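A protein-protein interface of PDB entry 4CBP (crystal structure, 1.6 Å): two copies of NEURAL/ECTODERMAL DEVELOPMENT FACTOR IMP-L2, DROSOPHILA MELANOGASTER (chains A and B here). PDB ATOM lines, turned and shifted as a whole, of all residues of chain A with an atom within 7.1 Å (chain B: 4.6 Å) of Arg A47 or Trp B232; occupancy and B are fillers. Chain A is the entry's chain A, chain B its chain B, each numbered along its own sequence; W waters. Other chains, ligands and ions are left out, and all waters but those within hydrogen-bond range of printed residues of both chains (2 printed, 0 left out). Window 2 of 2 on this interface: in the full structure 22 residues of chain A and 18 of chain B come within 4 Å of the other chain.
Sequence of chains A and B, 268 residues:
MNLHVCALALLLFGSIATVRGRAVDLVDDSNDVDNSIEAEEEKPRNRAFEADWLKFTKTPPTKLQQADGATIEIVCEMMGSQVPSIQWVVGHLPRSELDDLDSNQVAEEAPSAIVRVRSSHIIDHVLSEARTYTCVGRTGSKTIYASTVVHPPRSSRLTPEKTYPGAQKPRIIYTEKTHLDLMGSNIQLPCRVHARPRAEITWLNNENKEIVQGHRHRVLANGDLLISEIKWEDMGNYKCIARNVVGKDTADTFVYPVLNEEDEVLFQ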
ATOM      1  N   PRO A  44      -3.794  10.971   1.098  1.00  0.00           N
ATOM      2  CA  PRO A  44      -2.871  11.535   0.106  1.00  0.00           C
ATOM      3  C   PRO A  44      -3.586  11.770  -1.221  1.00  0.00           C
ATOM      4  O   PRO A  44      -3.035  11.696  -2.320  1.00  0.00           O
ATOM      5  CB  PRO A  44      -1.798  10.462   0.002  1.00  0.00           C
ATOM      6  CG  PRO A  44      -1.729   9.938   1.420  1.00  0.00           C
ATOM      7  CD  PRO A  44      -3.152   9.914   1.901  1.00  0.00           C
ATOM      8  N   ARG A  45      -4.853  12.111  -1.047  1.00  0.00           N
ATOM      9  CA  ARG A  45      -5.898  12.273  -2.056  1.00  0.00           C
ATOM     10  C   ARG A  45      -5.740  11.803  -3.513  1.00  0.00           C
ATOM     11  O   ARG A  45      -6.623  12.079  -4.313  1.00  0.00           O
ATOM     12  CB  ARG A  45      -6.314  13.747  -2.086  1.00  0.00           C
ATOM     13  CG  ARG A  45      -5.331  14.703  -2.715  1.00  0.00           C
ATOM     14  CD  ARG A  45      -5.873  16.116  -2.559  1.00  0.00           C
ATOM     15  NE  ARG A  45      -6.059  16.453  -1.147  1.00  0.00           N
ATOM     16  CZ  ARG A  45      -6.628  17.569  -0.704  1.00  0.00           C
ATOM     17  NH1 ARG A  45      -7.081  18.474  -1.562  1.00  0.00           N
ATOM     18  NH2 ARG A  45      -6.749  17.780   0.599  1.00  0.00           N
ATOM     19  N   ASN A  46      -4.683  11.095  -3.892  1.00  0.00           N
ATOM     20  CA  ASN A  46      -4.939  10.090  -4.916  1.00  0.00           C
ATOM     21  C   ASN A  46      -5.527   8.985  -4.077  1.00  0.00           C
ATOM     22  O   ASN A  46      -5.002   8.675  -3.006  1.00  0.00           O
ATOM     23  CB  ASN A  46      -3.713   9.624  -5.702  1.00  0.00           C
ATOM     24  CG  ASN A  46      -4.075   8.625  -6.799  1.00  0.00           C
ATOM     25  OD1 ASN A  46      -4.721   7.604  -6.545  1.00  0.00           O
ATOM     26  ND2 ASN A  46      -3.678   8.928  -8.029  1.00  0.00           N
ATOM     27  N   ARG A  47      -6.640   8.427  -4.534  1.00  0.00           N
ATOM     28  CA  ARG A  47      -7.398   7.492  -3.724  1.00  0.00           C
ATOM     29  C   ARG A  47      -6.589   6.232  -3.418  1.00  0.00           C
ATOM     30  O   ARG A  47      -6.870   5.522  -2.455  1.00  0.00           O
ATOM     31  CB  ARG A  47      -8.707   7.142  -4.434  1.00  0.00           C
ATOM     32  CG  ARG A  47      -9.723   6.413  -3.581  1.00  0.00           C
ATOM     33  CD  ARG A  47     -10.008   7.136  -2.272  1.00  0.00           C
ATOM     34  NE  ARG A  47     -10.395   8.530  -2.463  1.00  0.00           N
ATOM     35  CZ  ARG A  47     -10.930   9.291  -1.511  1.00  0.00           C
ATOM     36  NH1 ARG A  47     -11.159   8.786  -0.305  1.00  0.00           N
ATOM     37  NH2 ARG A  47     -11.245  10.556  -1.764  1.00  0.00           N
ATOM     38  N   ALA A  48      -5.569   5.979  -4.230  1.00  0.00           N
ATOM     39  CA  ALA A  48      -4.726   4.793  -4.080  1.00  0.00           C
ATOM     40  C   ALA A  48      -4.000   4.723  -2.734  1.00  0.00           C
ATOM     41  O   ALA A  48      -3.525   3.663  -2.342  1.00  0.00           O
ATOM     42  CB  ALA A  48      -3.705   4.739  -5.209  1.00  0.00           C
ATOM     43  N   PHE A  49      -3.896   5.849  -2.033  1.00  0.00           N
ATOM     44  CA  PHE A  49      -3.156   5.863  -0.777  1.00  0.00           C
ATOM     45  C   PHE A  49      -4.043   5.821   0.471  1.00  0.00           C
ATOM     46  O   PHE A  49      -3.552   6.021   1.575  1.00  0.00           O
ATOM     47  CB  PHE A  49      -2.253   7.102  -0.711  1.00  0.00           C
ATOM     48  CG  PHE A  49      -1.260   7.186  -1.832  1.00  0.00           C
ATOM     49  CD1 PHE A  49      -0.181   6.320  -1.879  1.00  0.00           C
ATOM     50  CD2 PHE A  49      -1.404   8.125  -2.836  1.00  0.00           C
ATOM     51  CE1 PHE A  49       0.730   6.384  -2.913  1.00  0.00           C
ATOM     52  CE2 PHE A  49      -0.494   8.198  -3.873  1.00  0.00           C
ATOM     53  CZ  PHE A  49       0.572   7.322  -3.912  1.00  0.00           C
ATOM     54  N   GLU A  50      -5.337   5.543   0.304  1.00  0.00           N
ATOM     55  CA  GLU A  50      -6.293   5.620   1.419  1.00  0.00           C
ATOM     56  C   GLU A  50      -6.808   4.283   1.987  1.00  0.00           C
ATOM     57  O   GLU A  50      -7.906   4.247   2.560  1.00  0.00           O
ATOM     58  CB  GLU A  50      -7.521   6.442   0.997  1.00  0.00           C
ATOM     59  CG  GLU A  50      -7.234   7.763   0.297  1.00  0.00           C
ATOM     60  CD  GLU A  50      -6.812   8.872   1.246  1.00  0.00           C
ATOM     61  OE1 GLU A  50      -6.805   8.654   2.477  1.00  0.00           O
ATOM     62  OE2 GLU A  50      -6.488   9.975   0.754  1.00  0.00           O
ATOM     63  N   ALA A  51      -6.063   3.191   1.841  1.00  0.00           N
ATOM     64  CA  ALA A  51      -6.503   1.920   2.443  1.00  0.00           C
ATOM     65  C   ALA A  51      -6.520   2.050   3.966  1.00  0.00           C
ATOM     66  O   ALA A  51      -5.642   2.707   4.526  1.00  0.00           O
ATOM     67  CB  ALA A  51      -5.591   0.768   2.014  1.00  0.00           C
ATOM     68  N   TRP A  53     -10.465   1.388   2.715  1.00  0.00           N
ATOM     69  CA  TRP A  53     -11.760   2.027   2.523  1.00  0.00           C
ATOM     70  C   TRP A  53     -12.654   1.136   1.670  1.00  0.00           C
ATOM     71  O   TRP A  53     -12.164   0.332   0.874  1.00  0.00           O
ATOM     72  CB  TRP A  53     -11.610   3.410   1.882  1.00  0.00           C
ATOM     73  CG  TRP A  53     -11.096   3.385   0.478  1.00  0.00           C
ATOM     74  CD1 TRP A  53      -9.791   3.346   0.085  1.00  0.00           C
ATOM     75  CD2 TRP A  53     -11.879   3.409  -0.726  1.00  0.00           C
ATOM     76  NE1 TRP A  53      -9.711   3.342  -1.289  1.00  0.00           N
ATOM     77  CE2 TRP A  53     -10.978   3.376  -1.810  1.00  0.00           C
ATOM     78  CE3 TRP A  53     -13.254   3.455  -0.991  1.00  0.00           C
ATOM     79  CZ2 TRP A  53     -11.405   3.387  -3.141  1.00  0.00           C
ATOM     80  CZ3 TRP A  53     -13.677   3.466  -2.315  1.00  0.00           C
ATOM     81  CH2 TRP A  53     -12.755   3.432  -3.372  1.00  0.00           C
ATOM     82  N   LYS A  55     -16.908   1.122  -0.040  1.00  0.00           N
ATOM     83  CA  LYS A  55     -18.182   1.811  -0.230  1.00  0.00           C
ATOM     84  C   LYS A  55     -19.108   0.997  -1.124  1.00  0.00           C
ATOM     85  O   LYS A  55     -18.661   0.490  -2.150  1.00  0.00           O
ATOM     86  CB  LYS A  55     -17.945   3.188  -0.856  1.00  0.00           C
ATOM     87  CG  LYS A  55     -19.200   4.026  -1.060  1.00  0.00           C
ATOM     88  CD  LYS A  55     -18.906   5.255  -1.926  1.00  0.00           C
ATOM     89  CE  LYS A  55     -20.102   6.199  -1.979  1.00  0.00           C
ATOM     90  NZ  LYS A  55     -19.932   7.300  -2.974  1.00  0.00           N
ATOM     91  N   MET A  79     -16.942  -0.828  -4.054  1.00  0.00           N
ATOM     92  CA  MET A  79     -15.607  -0.493  -4.511  1.00  0.00           C
ATOM     93  C   MET A  79     -14.762  -0.147  -3.303  1.00  0.00           C
ATOM     94  O   MET A  79     -15.252   0.472  -2.353  1.00  0.00           O
ATOM     95  CB  MET A  79     -15.639   0.675  -5.487  1.00  0.00           C
ATOM     96  CG  MET A  79     -14.316   0.908  -6.187  1.00  0.00           C
ATOM     97  SD  MET A  79     -14.504   2.360  -7.459  1.00  0.00           S
ATOM     98  CE  MET A  79     -13.165   1.831  -8.783  1.00  0.00           C
ATOM     99  N   SER A  81     -10.340  -0.301  -1.462  1.00  0.00           N
ATOM    100  CA  SER A  81      -8.913  -0.577  -1.593  1.00  0.00           C
ATOM    101  C   SER A  81      -8.621  -2.076  -1.685  1.00  0.00           C
ATOM    102  O   SER A  81      -9.418  -2.909  -1.222  1.00  0.00           O
ATOM    103  CB  SER A  81      -8.147   0.037  -0.417  1.00  0.00           C
ATOM    104  OG  SER A  81      -8.757  -0.300   0.825  1.00  0.00           O
ATOM    105  N   PRO A 111       0.885   2.632  -2.204  1.00  0.00           N
ATOM    106  CA  PRO A 111      -0.428   2.655  -2.854  1.00  0.00           C
ATOM    107  C   PRO A 111      -1.030   1.265  -2.901  1.00  0.00           C
ATOM    108  O   PRO A 111      -0.317   0.267  -2.791  1.00  0.00           O
ATOM    109  CB  PRO A 111      -0.115   3.159  -4.261  1.00  0.00           C
ATOM    110  CG  PRO A 111       1.299   2.686  -4.506  1.00  0.00           C
ATOM    111  CD  PRO A 111       1.984   2.830  -3.169  1.00  0.00           C
ATOM    112  N   SER A 112      -2.343   1.210  -3.056  1.00  0.00           N
ATOM    113  CA  SER A 112      -3.033  -0.058  -3.210  1.00  0.00           C
ATOM    114  C   SER A 112      -3.806  -0.078  -4.507  1.00  0.00           C
ATOM    115  O   SER A 112      -4.033   0.962  -5.126  1.00  0.00           O
ATOM    116  CB  SER A 112      -4.002  -0.299  -2.054  1.00  0.00           C
ATOM    117  OG  SER A 112      -5.162   0.502  -2.220  1.00  0.00           O
ATOM    118  N   ALA A 113      -4.222  -1.274  -4.901  1.00  0.00           N
ATOM    119  CA  ALA A 113      -5.197  -1.420  -5.966  1.00  0.00           C
ATOM    120  C   ALA A 113      -6.523  -0.817  -5.515  1.00  0.00           C
ATOM    121  O   ALA A 113      -6.746  -0.594  -4.323  1.00  0.00           O
ATOM    122  CB  ALA A 113      -5.375  -2.894  -6.338  1.00  0.00           C
ATOM    123  N   ILE A 114      -7.389  -0.539  -6.478  1.00  0.00           N
ATOM    124  CA  ILE A 114      -8.752  -0.131  -6.181  1.00  0.00           C
ATOM    125  C   ILE A 114      -9.650  -0.984  -7.065  1.00  0.00           C
ATOM    126  O   ILE A 114      -9.485  -0.988  -8.277  1.00  0.00           O
ATOM    127  CB  ILE A 114      -8.995   1.359  -6.449  1.00  0.00           C
ATOM    128  CG1 ILE A 114      -8.178   2.213  -5.466  1.00  0.00           C
ATOM    129  CG2 ILE A 114     -10.473   1.691  -6.294  1.00  0.00           C
ATOM    130  CD1 ILE A 114      -8.179   3.690  -5.789  1.00  0.00           C
ATOM    131  N   VAL A 258      -3.704   2.335 -11.522  1.00  0.00           N
ATOM    132  CA  VAL A 258      -4.304   3.152 -10.477  1.00  0.00           C
ATOM    133  C   VAL A 258      -3.515   4.456 -10.309  1.00  0.00           C
ATOM    134  O   VAL A 258      -4.092   5.481  -9.945  1.00  0.00           O
ATOM    135  CB  VAL A 258      -4.400   2.372  -9.134  1.00  0.00           C
ATOM    136  CG1 VAL A 258      -3.024   2.160  -8.509  1.00  0.00           C
ATOM    137  CG2 VAL A 258      -5.368   3.061  -8.169  1.00  0.00           C
ATOM    138  N   LEU A 259      -2.217   4.416 -10.629  1.00  0.00           N
ATOM    139  CA  LEU A 259      -1.332   5.582 -10.505  1.00  0.00           C
ATOM    140  C   LEU A 259      -0.631   5.963 -11.807  1.00  0.00           C
ATOM    141  O   LEU A 259      -0.636   5.201 -12.774  1.00  0.00           O
ATOM    142  CB  LEU A 259      -0.251   5.337  -9.446  1.00  0.00           C
ATOM    143  CG  LEU A 259      -0.624   5.335  -7.966  1.00  0.00           C
ATOM    144  CD1 LEU A 259       0.632   5.195  -7.129  1.00  0.00           C
ATOM    145  CD2 LEU A 259      -1.363   6.607  -7.599  1.00  0.00           C
ATOM    146  N   MET B 183     -12.328  15.597 -11.066  1.00  0.00           N
ATOM    147  CA  MET B 183     -12.855  16.357  -9.936  1.00  0.00           C
ATOM    148  C   MET B 183     -13.004  17.823 -10.302  1.00  0.00           C
ATOM    149  O   MET B 183     -12.081  18.417 -10.855  1.00  0.00           O
ATOM    150  CB  MET B 183     -11.932  16.259  -8.724  1.00  0.00           C
ATOM    151  CG  MET B 183     -11.675  14.872  -8.235  1.00  0.00           C
ATOM    152  SD  MET B 183     -12.721  14.487  -6.674  1.00  0.00           S
ATOM    153  CE  MET B 183     -11.675  12.984  -6.006  1.00  0.00           C
ATOM    154  N   LYS B 231     -17.445  15.881  -7.147  1.00  0.00           N
ATOM    155  CA  LYS B 231     -16.540  15.653  -6.031  1.00  0.00           C
ATOM    156  C   LYS B 231     -16.510  14.165  -5.718  1.00  0.00           C
ATOM    157  O   LYS B 231     -17.273  13.396  -6.307  1.00  0.00           O
ATOM    158  CB  LYS B 231     -16.968  16.467  -4.812  1.00  0.00           C
ATOM    159  CG  LYS B 231     -18.436  16.339  -4.456  1.00  0.00           C
ATOM    160  CD  LYS B 231     -18.801  17.328  -3.352  1.00  0.00           C
ATOM    161  CE  LYS B 231     -20.271  17.233  -2.971  1.00  0.00           C
ATOM    162  NZ  LYS B 231     -20.608  18.190  -1.876  1.00  0.00           N
ATOM    163  N   TRP B 232     -15.638  13.757  -4.799  1.00  0.00           N
ATOM    164  CA  TRP B 232     -15.472  12.333  -4.526  1.00  0.00           C
ATOM    165  C   TRP B 232     -16.781  11.698  -4.056  1.00  0.00           C
ATOM    166  O   TRP B 232     -17.089  10.552  -4.402  1.00  0.00           O
ATOM    167  CB  TRP B 232     -14.368  12.103  -3.493  1.00  0.00           C
ATOM    168  CG  TRP B 232     -14.246  10.663  -3.082  1.00  0.00           C
ATOM    169  CD1 TRP B 232     -14.487  10.145  -1.845  1.00  0.00           C
ATOM    170  CD2 TRP B 232     -13.870   9.556  -3.916  1.00  0.00           C
ATOM    171  NE1 TRP B 232     -14.283   8.782  -1.851  1.00  0.00           N
ATOM    172  CE2 TRP B 232     -13.907   8.396  -3.113  1.00  0.00           C
ATOM    173  CE3 TRP B 232     -13.504   9.433  -5.261  1.00  0.00           C
ATOM    174  CZ2 TRP B 232     -13.580   7.132  -3.605  1.00  0.00           C
ATOM    175  CZ3 TRP B 232     -13.184   8.172  -5.753  1.00  0.00           C
ATOM    176  CH2 TRP B 232     -13.225   7.040  -4.925  1.00  0.00           C
ATOM    177  N   GLU B 233     -17.567  12.458  -3.301  1.00  0.00           N
ATOM    178  CA  GLU B 233     -18.830  11.959  -2.766  1.00  0.00           C
ATOM    179  C   GLU B 233     -19.855  11.645  -3.859  1.00  0.00           C
ATOM    180  O   GLU B 233     -20.860  10.976  -3.594  1.00  0.00           O
ATOM    181  CB  GLU B 233     -19.425  12.964  -1.775  1.00  0.00           C
ATOM    182  CG  GLU B 233     -18.680  13.064  -0.438  1.00  0.00           C
ATOM    183  CD  GLU B 233     -17.339  13.804  -0.509  1.00  0.00           C
ATOM    184  OE1 GLU B 233     -17.082  14.545  -1.486  1.00  0.00           O
ATOM    185  OE2 GLU B 233     -16.538  13.648   0.440  1.00  0.00           O
ATOM    186  N   ASP B 234     -19.600  12.120  -5.081  1.00  0.00           N
ATOM    187  CA  ASP B 234     -20.473  11.825  -6.216  1.00  0.00           C
ATOM    188  C   ASP B 234     -20.175  10.461  -6.842  1.00  0.00           C
ATOM    189  O   ASP B 234     -20.922   9.993  -7.712  1.00  0.00           O
ATOM    190  CB  ASP B 234     -20.342  12.899  -7.296  1.00  0.00           C
ATOM    191  CG  ASP B 234     -20.840  14.254  -6.845  1.00  0.00           C
ATOM    192  OD1 ASP B 234     -21.851  14.332  -6.103  1.00  0.00           O
ATOM    193  OD2 ASP B 234     -20.216  15.250  -7.246  1.00  0.00           O
ATOM    194  N   MET B 235     -19.090   9.824  -6.407  1.00  0.00           N
ATOM    195  CA  MET B 235     -18.709   8.524  -6.953  1.00  0.00           C
ATOM    196  C   MET B 235     -19.823   7.504  -6.751  1.00  0.00           C
ATOM    197  O   MET B 235     -20.441   7.451  -5.682  1.00  0.00           O
ATOM    198  CB  MET B 235     -17.409   8.023  -6.306  1.00  0.00           C
ATOM    199  CG  MET B 235     -16.866   6.739  -6.916  1.00  0.00           C
ATOM    200  SD  MET B 235     -17.600   5.083  -6.122  1.00  0.00           S
ATOM    201  CE  MET B 235     -16.348   4.895  -4.611  1.00  0.00           C
ATOM    202  N   TYR B 256     -16.809   7.900 -11.735  1.00  0.00           N
ATOM    203  CA  TYR B 256     -15.584   7.785 -10.947  1.00  0.00           C
ATOM    204  C   TYR B 256     -14.759   9.067 -11.056  1.00  0.00           C
ATOM    205  O   TYR B 256     -14.097   9.305 -12.068  1.00  0.00           O
ATOM    206  CB  TYR B 256     -14.754   6.571 -11.401  1.00  0.00           C
ATOM    207  CG  TYR B 256     -13.611   6.257 -10.454  1.00  0.00           C
ATOM    208  CD1 TYR B 256     -13.856   5.703  -9.198  1.00  0.00           C
ATOM    209  CD2 TYR B 256     -12.294   6.522 -10.806  1.00  0.00           C
ATOM    210  CE1 TYR B 256     -12.823   5.421  -8.321  1.00  0.00           C
ATOM    211  CE2 TYR B 256     -11.248   6.241  -9.925  1.00  0.00           C
ATOM    212  CZ  TYR B 256     -11.521   5.697  -8.687  1.00  0.00           C
ATOM    213  OH  TYR B 256     -10.491   5.412  -7.810  1.00  0.00           O
ATOM    214  N   PRO B 257     -14.804   9.906 -10.010  1.00  0.00           N
ATOM    215  CA  PRO B 257     -14.066  11.170 -10.020  1.00  0.00           C
ATOM    216  C   PRO B 257     -12.581  10.948  -9.770  1.00  0.00           C
ATOM    217  O   PRO B 257     -12.217  10.225  -8.836  1.00  0.00           O
ATOM    218  CB  PRO B 257     -14.704  11.965  -8.867  1.00  0.00           C
ATOM    219  CG  PRO B 257     -15.985  11.219  -8.512  1.00  0.00           C
ATOM    220  CD  PRO B 257     -15.670   9.791  -8.829  1.00  0.00           C
HETATM  221  O   HOH W   1     -17.494   8.317  -2.614  1.00  0.00           O
HETATM  222  O   HOH W   2     -21.487   9.162  -1.459  1.00  0.00           O
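No position is printed for both chains. Of the 7 pairs that touch across the chains among the printed residues, none has its exchanged pair printed and touching as well.
Among the printed residues, pairs that only touch across the chains: Ile A114 with Tyr B256 (3.5 Å), Met A79 with Tyr B256 (3.6 Å), Trp A53 with Trp B232 (3.8 Å), Trp A53 with Met B235 (3.8 Å) and Lys A55 with Glu B233 (3.8 Å).
Arg A47 touches just one residue of chain B: Trp B232 (3.3 Å). Of chain A, only Arg A47 (3.3 Å) and Trp A53 (3.8 Å) come within 4 Å of Trp B232. Printed residues of chain A within 4 Å of Glu B233: Lys A55 (3.8 Å). Of the printed residues of chain A, Met B235 touches Trp A53 and Lys A55. Printed residues of chain B within 4 Å of Trp A53: Trp B232 (3.8 Å) and Met B235 (3.8 Å). Phe A49 touches none of the printed residues of chain B. Ser A81 touches none of the printed residues of chain B.
Water W1 lies within hydrogen-bond range of NZ of Lys A55 (2.7 Å) and O of Trp B232 (2.9 Å). Water W2 lies within hydrogen-bond range of the side-chain amino group (NZ) of Lys A55 (2.9 Å) and the backbone carbonyl oxygen (O) of Glu B233 (2.9 Å).
NZ of Lys A55 is in hydrogen-bond range of O of Met B235, at 2.8 Å. NH1 of Arg A47 lies close to NE1 of Trp B232 (3.5 Å).
O of Trp A53 lies within hydrogen-bond range of N of Ser A81, at 3.0 Å. The backbone carbonyl oxygen of Lys A55 sits at hydrogen-bond distance from the backbone NH of Met A79 (2.9 Å). N of Trp B232 is in hydrogen-bond range of SD of Met B183 (3.5 Å).
Hydrophobic or aromatic side chains of chain B that line the printed part of chain A: Trp B232, Met B235 and Tyr B256. Hydrophobic or aromatic side chains of chain A that line the printed part of chain B: Trp A53, Met A79 and Ile A114. Among the printed residues, 7 pairs touch across the chains.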
